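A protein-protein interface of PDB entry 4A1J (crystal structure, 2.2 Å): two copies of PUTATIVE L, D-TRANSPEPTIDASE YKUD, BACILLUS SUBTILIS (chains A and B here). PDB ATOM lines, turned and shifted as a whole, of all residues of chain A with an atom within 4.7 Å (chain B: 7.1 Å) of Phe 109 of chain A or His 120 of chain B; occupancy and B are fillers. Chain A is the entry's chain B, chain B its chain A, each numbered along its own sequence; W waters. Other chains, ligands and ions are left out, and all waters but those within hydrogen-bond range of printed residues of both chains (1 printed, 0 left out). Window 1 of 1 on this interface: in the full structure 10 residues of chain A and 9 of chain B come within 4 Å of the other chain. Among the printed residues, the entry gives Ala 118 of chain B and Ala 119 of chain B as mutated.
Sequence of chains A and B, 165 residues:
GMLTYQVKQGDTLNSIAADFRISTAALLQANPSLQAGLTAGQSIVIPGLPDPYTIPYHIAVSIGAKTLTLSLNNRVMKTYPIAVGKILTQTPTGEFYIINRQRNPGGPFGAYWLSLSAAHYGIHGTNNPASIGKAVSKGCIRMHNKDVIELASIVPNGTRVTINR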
ATOM      1  N   GLN A 102       4.117   5.313  17.149  1.00  0.00           N
ATOM      2  CA  GLN A 102       3.831   6.583  17.787  1.00  0.00           C
ATOM      3  C   GLN A 102       4.767   7.610  17.186  1.00  0.00           C
ATOM      4  O   GLN A 102       5.970   7.373  17.096  1.00  0.00           O
ATOM      5  CB  GLN A 102       4.037   6.515  19.308  1.00  0.00           C
ATOM      6  CG  GLN A 102       3.072   5.574  20.039  1.00  0.00           C
ATOM      7  CD  GLN A 102       3.429   4.088  19.881  1.00  0.00           C
ATOM      8  OE1 GLN A 102       2.617   3.293  19.403  1.00  0.00           O
ATOM      9  NE2 GLN A 102       4.636   3.713  20.294  1.00  0.00           N
ATOM     10  N   PRO A 105       7.987  10.376  19.782  1.00  0.00           N
ATOM     11  CA  PRO A 105       8.069   9.944  21.184  1.00  0.00           C
ATOM     12  C   PRO A 105       9.148  10.711  21.962  1.00  0.00           C
ATOM     13  O   PRO A 105       9.132  10.732  23.195  1.00  0.00           O
ATOM     14  CB  PRO A 105       8.448   8.475  21.065  1.00  0.00           C
ATOM     15  CG  PRO A 105       9.172   8.391  19.732  1.00  0.00           C
ATOM     16  CD  PRO A 105       8.387   9.308  18.853  1.00  0.00           C
ATOM     17  N   GLY A 106      10.072  11.340  21.242  1.00  0.00           N
ATOM     18  CA  GLY A 106      11.106  12.157  21.864  1.00  0.00           C
ATOM     19  C   GLY A 106      12.141  11.392  22.673  1.00  0.00           C
ATOM     20  O   GLY A 106      12.224  10.159  22.609  1.00  0.00           O
ATOM     21  N   GLY A 107      12.926  12.126  23.454  1.00  0.00           N
ATOM     22  CA  GLY A 107      14.051  11.545  24.168  1.00  0.00           C
ATOM     23  C   GLY A 107      14.917  10.681  23.262  1.00  0.00           C
ATOM     24  O   GLY A 107      15.135  11.009  22.093  1.00  0.00           O
ATOM     25  N   PRO A 108      15.411   9.557  23.793  1.00  0.00           N
ATOM     26  CA  PRO A 108      16.286   8.703  22.994  1.00  0.00           C
ATOM     27  C   PRO A 108      15.569   8.054  21.818  1.00  0.00           C
ATOM     28  O   PRO A 108      16.234   7.425  21.004  1.00  0.00           O
ATOM     29  CB  PRO A 108      16.759   7.639  23.999  1.00  0.00           C
ATOM     30  CG  PRO A 108      15.752   7.645  25.078  1.00  0.00           C
ATOM     31  CD  PRO A 108      15.243   9.054  25.167  1.00  0.00           C
ATOM     32  N   PHE A 109      14.252   8.216  21.719  1.00  0.00           N
ATOM     33  CA  PHE A 109      13.485   7.535  20.678  1.00  0.00           C
ATOM     34  C   PHE A 109      13.248   8.395  19.436  1.00  0.00           C
ATOM     35  O   PHE A 109      12.764   7.892  18.425  1.00  0.00           O
ATOM     36  CB  PHE A 109      12.159   6.986  21.232  1.00  0.00           C
ATOM     37  CG  PHE A 109      12.321   6.201  22.504  1.00  0.00           C
ATOM     38  CD1 PHE A 109      12.955   4.967  22.495  1.00  0.00           C
ATOM     39  CD2 PHE A 109      11.869   6.712  23.715  1.00  0.00           C
ATOM     40  CE1 PHE A 109      13.126   4.247  23.672  1.00  0.00           C
ATOM     41  CE2 PHE A 109      12.035   6.005  24.894  1.00  0.00           C
ATOM     42  CZ  PHE A 109      12.670   4.767  24.876  1.00  0.00           C
ATOM     43  N   GLY A 110      13.585   9.681  19.512  1.00  0.00           N
ATOM     44  CA  GLY A 110      13.523  10.564  18.354  1.00  0.00           C
ATOM     45  C   GLY A 110      12.174  10.745  17.660  1.00  0.00           C
ATOM     46  O   GLY A 110      11.130  10.890  18.304  1.00  0.00           O
ATOM     47  N   ALA A 111      12.197  10.741  16.330  1.00  0.00           N
ATOM     48  CA  ALA A 111      11.055  11.210  15.545  1.00  0.00           C
ATOM     49  C   ALA A 111       9.905  10.195  15.454  1.00  0.00           C
ATOM     50  O   ALA A 111       8.765  10.553  15.179  1.00  0.00           O
ATOM     51  CB  ALA A 111      11.515  11.621  14.151  1.00  0.00           C
ATOM     52  N   TYR A 112      10.206   8.927  15.678  1.00  0.00           N
ATOM     53  CA  TYR A 112       9.207   7.894  15.500  1.00  0.00           C
ATOM     54  C   TYR A 112       9.542   6.651  16.303  1.00  0.00           C
ATOM     55  O   TYR A 112      10.714   6.370  16.591  1.00  0.00           O
ATOM     56  CB  TYR A 112       9.029   7.553  14.005  1.00  0.00           C
ATOM     57  CG  TYR A 112       7.630   7.822  13.489  1.00  0.00           C
ATOM     58  CD1 TYR A 112       6.590   6.958  13.788  1.00  0.00           C
ATOM     59  CD2 TYR A 112       7.343   8.951  12.718  1.00  0.00           C
ATOM     60  CE1 TYR A 112       5.301   7.193  13.341  1.00  0.00           C
ATOM     61  CE2 TYR A 112       6.046   9.194  12.255  1.00  0.00           C
ATOM     62  CZ  TYR A 112       5.032   8.307  12.576  1.00  0.00           C
ATOM     63  OH  TYR A 112       3.734   8.515  12.144  1.00  0.00           O
ATOM     64  N   TRP A 113       8.504   5.921  16.689  1.00  0.00           N
ATOM     65  CA  TRP A 113       8.673   4.571  17.220  1.00  0.00           C
ATOM     66  C   TRP A 113       7.764   3.631  16.436  1.00  0.00           C
ATOM     67  O   TRP A 113       6.561   3.876  16.324  1.00  0.00           O
ATOM     68  CB  TRP A 113       8.335   4.520  18.717  1.00  0.00           C
ATOM     69  CG  TRP A 113       8.229   3.102  19.260  1.00  0.00           C
ATOM     70  CD1 TRP A 113       7.163   2.258  19.133  1.00  0.00           C
ATOM     71  CD2 TRP A 113       9.224   2.373  20.007  1.00  0.00           C
ATOM     72  NE1 TRP A 113       7.425   1.062  19.749  1.00  0.00           N
ATOM     73  CE2 TRP A 113       8.685   1.097  20.284  1.00  0.00           C
ATOM     74  CE3 TRP A 113      10.509   2.676  20.467  1.00  0.00           C
ATOM     75  CZ2 TRP A 113       9.381   0.126  21.005  1.00  0.00           C
ATOM     76  CZ3 TRP A 113      11.206   1.708  21.178  1.00  0.00           C
ATOM     77  CH2 TRP A 113      10.639   0.452  21.444  1.00  0.00           C
ATOM     78  N   HIS A 124      13.270   2.687  15.940  1.00  0.00           N
ATOM     79  CA  HIS A 124      13.021   4.057  16.346  1.00  0.00           C
ATOM     80  C   HIS A 124      14.082   5.013  15.862  1.00  0.00           C
ATOM     81  O   HIS A 124      15.065   4.591  15.265  1.00  0.00           O
ATOM     82  CB  HIS A 124      12.762   4.175  17.856  1.00  0.00           C
ATOM     83  CG  HIS A 124      13.911   3.780  18.734  1.00  0.00           C
ATOM     84  ND1 HIS A 124      15.054   4.539  18.858  1.00  0.00           N
ATOM     85  CD2 HIS A 124      14.055   2.746  19.597  1.00  0.00           C
ATOM     86  CE1 HIS A 124      15.866   3.971  19.731  1.00  0.00           C
ATOM     87  NE2 HIS A 124      15.281   2.887  20.200  1.00  0.00           N
ATOM     88  N   GLY A 125      13.829   6.303  16.063  1.00  0.00           N
ATOM     89  CA  GLY A 125      14.789   7.348  15.771  1.00  0.00           C
ATOM     90  C   GLY A 125      15.830   7.383  16.873  1.00  0.00           C
ATOM     91  O   GLY A 125      15.973   6.419  17.632  1.00  0.00           O
ATOM     92  N   THR A 126      16.562   8.488  16.964  1.00  0.00           N
ATOM     93  CA  THR A 126      17.572   8.631  17.992  1.00  0.00           C
ATOM     94  C   THR A 126      17.825  10.110  18.268  1.00  0.00           C
ATOM     95  O   THR A 126      17.530  10.955  17.429  1.00  0.00           O
ATOM     96  CB  THR A 126      18.911   7.989  17.555  1.00  0.00           C
ATOM     97  OG1 THR A 126      19.791   7.899  18.683  1.00  0.00           O
ATOM     98  CG2 THR A 126      19.581   8.839  16.470  1.00  0.00           C
ATOM     99  N   ALA B  18      -0.123   3.719  24.048  1.00  0.00           N
ATOM    100  CA  ALA B  18       1.256   3.291  24.295  1.00  0.00           C
ATOM    101  C   ALA B  18       1.691   3.511  25.758  1.00  0.00           C
ATOM    102  O   ALA B  18       2.351   2.656  26.350  1.00  0.00           O
ATOM    103  CB  ALA B  18       2.203   3.984  23.349  1.00  0.00           C
ATOM    104  N   ASP B  19       1.320   4.648  26.340  1.00  0.00           N
ATOM    105  CA  ASP B  19       1.674   4.927  27.733  1.00  0.00           C
ATOM    106  C   ASP B  19       1.078   3.911  28.714  1.00  0.00           C
ATOM    107  O   ASP B  19       1.736   3.498  29.665  1.00  0.00           O
ATOM    108  CB  ASP B  19       1.246   6.335  28.137  1.00  0.00           C
ATOM    109  CG  ASP B  19       2.216   7.395  27.670  1.00  0.00           C
ATOM    110  OD1 ASP B  19       3.292   7.042  27.136  1.00  0.00           O
ATOM    111  OD2 ASP B  19       1.909   8.590  27.850  1.00  0.00           O
ATOM    112  N   ARG B  21      -0.075   0.851  27.863  1.00  0.00           N
ATOM    113  CA  ARG B  21       0.140  -0.506  27.365  1.00  0.00           C
ATOM    114  C   ARG B  21      -1.153  -1.220  27.016  1.00  0.00           C
ATOM    115  O   ARG B  21      -1.340  -2.381  27.382  1.00  0.00           O
ATOM    116  CB  ARG B  21       0.941  -1.343  28.371  1.00  0.00           C
ATOM    117  CG  ARG B  21       2.207  -0.656  28.879  1.00  0.00           C
ATOM    118  CD  ARG B  21       3.190  -0.354  27.743  1.00  0.00           C
ATOM    119  NE  ARG B  21       4.536  -0.220  28.274  1.00  0.00           N
ATOM    120  CZ  ARG B  21       4.963   0.810  29.003  1.00  0.00           C
ATOM    121  NH1 ARG B  21       4.141   1.828  29.269  1.00  0.00           N
ATOM    122  NH2 ARG B  21       6.213   0.817  29.474  1.00  0.00           N
ATOM    123  N   TRP B 113       9.951  -7.555  34.933  1.00  0.00           N
ATOM    124  CA  TRP B 113       9.766  -6.237  34.341  1.00  0.00           C
ATOM    125  C   TRP B 113       8.391  -5.722  34.761  1.00  0.00           C
ATOM    126  O   TRP B 113       7.402  -6.448  34.693  1.00  0.00           O
ATOM    127  CB  TRP B 113       9.911  -6.275  32.815  1.00  0.00           C
ATOM    128  CG  TRP B 113       9.350  -5.049  32.150  1.00  0.00           C
ATOM    129  CD1 TRP B 113       8.025  -4.745  31.977  1.00  0.00           C
ATOM    130  CD2 TRP B 113      10.087  -3.960  31.580  1.00  0.00           C
ATOM    131  NE1 TRP B 113       7.894  -3.533  31.336  1.00  0.00           N
ATOM    132  CE2 TRP B 113       9.142  -3.034  31.074  1.00  0.00           C
ATOM    133  CE3 TRP B 113      11.452  -3.681  31.437  1.00  0.00           C
ATOM    134  CZ2 TRP B 113       9.519  -1.844  30.447  1.00  0.00           C
ATOM    135  CZ3 TRP B 113      11.828  -2.504  30.811  1.00  0.00           C
ATOM    136  CH2 TRP B 113      10.863  -1.593  30.327  1.00  0.00           C
ATOM    137  N   LEU B 116       5.860   1.048  33.610  1.00  0.00           N
ATOM    138  CA  LEU B 116       5.388   2.321  34.159  1.00  0.00           C
ATOM    139  C   LEU B 116       4.536   2.968  33.081  1.00  0.00           C
ATOM    140  O   LEU B 116       4.648   2.616  31.914  1.00  0.00           O
ATOM    141  CB  LEU B 116       6.556   3.252  34.520  1.00  0.00           C
ATOM    142  CG  LEU B 116       7.448   2.798  35.676  1.00  0.00           C
ATOM    143  CD1 LEU B 116       8.725   3.627  35.784  1.00  0.00           C
ATOM    144  CD2 LEU B 116       6.664   2.829  36.960  1.00  0.00           C
ATOM    145  N   SER B 117       3.691   3.910  33.479  1.00  0.00           N
ATOM    146  CA  SER B 117       2.740   4.547  32.576  1.00  0.00           C
ATOM    147  C   SER B 117       3.414   5.585  31.685  1.00  0.00           C
ATOM    148  O   SER B 117       2.814   6.595  31.326  1.00  0.00           O
ATOM    149  CB  SER B 117       1.615   5.202  33.375  1.00  0.00           C
ATOM    150  OG  SER B 117       2.151   6.107  34.330  1.00  0.00           O
ATOM    151  N   ALA B 118       4.677   5.355  31.357  1.00  0.00           N
ATOM    152  CA  ALA B 118       5.308   6.105  30.284  1.00  0.00           C
ATOM    153  C   ALA B 118       5.893   5.106  29.294  1.00  0.00           C
ATOM    154  O   ALA B 118       6.679   4.228  29.673  1.00  0.00           O
ATOM    155  CB  ALA B 118       6.380   7.055  30.826  1.00  0.00           C
ATOM    156  N   ALA B 119       5.492   5.234  28.032  1.00  0.00           N
ATOM    157  CA  ALA B 119       5.898   4.301  26.993  1.00  0.00           C
ATOM    158  C   ALA B 119       7.397   3.999  27.070  1.00  0.00           C
ATOM    159  O   ALA B 119       8.205   4.909  27.231  1.00  0.00           O
ATOM    160  CB  ALA B 119       5.539   4.868  25.603  1.00  0.00           C
ATOM    161  N   HIS B 120       7.747   2.720  26.939  1.00  0.00           N
ATOM    162  CA  HIS B 120       9.142   2.275  26.886  1.00  0.00           C
ATOM    163  C   HIS B 120       9.892   2.421  28.208  1.00  0.00           C
ATOM    164  O   HIS B 120      11.101   2.167  28.269  1.00  0.00           O
ATOM    165  CB  HIS B 120       9.912   3.028  25.802  1.00  0.00           C
ATOM    166  CG  HIS B 120       9.116   3.280  24.562  1.00  0.00           C
ATOM    167  ND1 HIS B 120       8.436   2.280  23.900  1.00  0.00           N
ATOM    168  CD2 HIS B 120       8.888   4.419  23.867  1.00  0.00           C
ATOM    169  CE1 HIS B 120       7.821   2.794  22.850  1.00  0.00           C
ATOM    170  NE2 HIS B 120       8.082   4.089  22.805  1.00  0.00           N
ATOM    171  N   TYR B 121       9.194   2.834  29.261  1.00  0.00           N
ATOM    172  CA  TYR B 121       9.824   2.878  30.574  1.00  0.00           C
ATOM    173  C   TYR B 121       9.265   1.853  31.541  1.00  0.00           C
ATOM    174  O   TYR B 121       8.082   1.531  31.501  1.00  0.00           O
ATOM    175  CB  TYR B 121       9.772   4.291  31.154  1.00  0.00           C
ATOM    176  CG  TYR B 121      10.684   5.200  30.387  1.00  0.00           C
ATOM    177  CD1 TYR B 121      12.060   5.110  30.545  1.00  0.00           C
ATOM    178  CD2 TYR B 121      10.187   6.092  29.447  1.00  0.00           C
ATOM    179  CE1 TYR B 121      12.914   5.911  29.826  1.00  0.00           C
ATOM    180  CE2 TYR B 121      11.035   6.904  28.730  1.00  0.00           C
ATOM    181  CZ  TYR B 121      12.404   6.807  28.922  1.00  0.00           C
ATOM    182  OH  TYR B 121      13.274   7.607  28.206  1.00  0.00           O
ATOM    183  N   GLY B 122      10.139   1.325  32.395  1.00  0.00           N
ATOM    184  CA  GLY B 122       9.736   0.377  33.414  1.00  0.00           C
ATOM    185  C   GLY B 122      10.738   0.247  34.551  1.00  0.00           C
ATOM    186  O   GLY B 122      11.782   0.892  34.561  1.00  0.00           O
ATOM    187  N   LYS B 138      19.529   3.455  30.524  1.00  0.00           N
ATOM    188  CA  LYS B 138      19.028   4.231  29.396  1.00  0.00           C
ATOM    189  C   LYS B 138      17.735   4.955  29.761  1.00  0.00           C
ATOM    190  O   LYS B 138      17.095   5.575  28.907  1.00  0.00           O
ATOM    191  CB  LYS B 138      18.839   3.353  28.146  1.00  0.00           C
ATOM    192  CG  LYS B 138      20.101   2.603  27.702  1.00  0.00           C
ATOM    193  CD  LYS B 138      19.920   1.953  26.328  1.00  0.00           C
ATOM    194  CE  LYS B 138      21.201   1.268  25.846  1.00  0.00           C
ATOM    195  NZ  LYS B 138      22.315   2.223  25.631  1.00  0.00           N
ATOM    196  N   GLY B 139      17.369   4.891  31.038  1.00  0.00           N
ATOM    197  CA  GLY B 139      16.228   5.635  31.543  1.00  0.00           C
ATOM    198  C   GLY B 139      15.353   4.778  32.433  1.00  0.00           C
ATOM    199  O   GLY B 139      14.591   5.297  33.260  1.00  0.00           O
ATOM    200  N   CYS B 140      15.447   3.460  32.260  1.00  0.00           N
ATOM    201  CA  CYS B 140      14.691   2.538  33.094  1.00  0.00           C
ATOM    202  C   CYS B 140      15.257   2.480  34.519  1.00  0.00           C
ATOM    203  O   CYS B 140      16.425   2.810  34.742  1.00  0.00           O
ATOM    204  CB  CYS B 140      14.647   1.146  32.453  1.00  0.00           C
ATOM    205  SG  CYS B 140      13.482   1.019  31.042  1.00  0.00           S
HETATM  206  O   HOH W   1       6.088   5.255  21.678  1.00  0.00           O
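N of Leu 116 of chain B lies within hydrogen-bond range of O of Tyr 121 of chain B (3.1 Å). The backbone carbonyl oxygen of Gln 102 of chain A sits at hydrogen-bond distance from the backbone NH of Trp 113 of chain A, 2.9 Å away. The backbone NH (N) of Gly 125 of chain A is in hydrogen-bond range of the backbone carbonyl oxygen (O) of Phe 109 of chain A (3.0 Å). The guanidinium group of Arg 21 of chain B is in hydrogen-bond range of the backbone carbonyl oxygen of Tyr 121 of chain B (2.8 Å).
Among the printed residues, merely in contact across the chains: Gln 102 of chain A with Ala 18 of chain B (3.7 Å), Pro 108 of chain A with Tyr 121 of chain B (3.9 Å), Phe 109 of chain A with His 120 of chain B (3.4 Å), Phe 109 of chain A with Tyr 121 of chain B (3.9 Å) and Trp 113 of chain A with His 120 of chain B (3.2 Å).
Of the printed residues of chain A, Tyr 121 of chain B touches Pro 108 and Phe 109. Of the printed residues of chain A, Ala 18 of chain B touches Gln 102 (3.7 Å). Of the printed residues of chain B, Pro 108 of chain A touches Tyr 121 (3.9 Å). Of the printed residues of chain B, Gln 102 of chain A touches Ala 18. Printed residues of chain B within 4 Å of Trp 113 of chain A: His 120 (3.2 Å). The nearest residue of chain B that does not touch Phe 109 of chain A is Ala 119 of chain B (4.6 Å).
Of the 13 printed residues of chain A, 4 touch a printed residue of chain B. Of the 14 printed residues of chain B, 3 touch a printed residue of chain A. Hydrophobic or aromatic side chains of chain B within 4 Å of the printed part of chain A: Ala 18, His 120 and Tyr 121. Along chain B the printed residues that touch a printed residue of chain A span positions 18 to 121. Among the printed residues, 5 pairs touch across the chains. Among the printed residues, no Asp or Glu carboxylate lies within 4 Å of a Lys or Arg side-chain nitrogen of the other chain.
1 position is printed for both chains. Of the 5 pairs that touch across the chains among the printed residues, none has its exchanged pair printed and touching as well.
Water W1 lies within hydrogen-bond range of the side-chain amide nitrogen (NE2) of Gln 102 of chain A (2.5 Å) and a ring nitrogen (NE2) of His 120 of chain B (2.6 Å).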
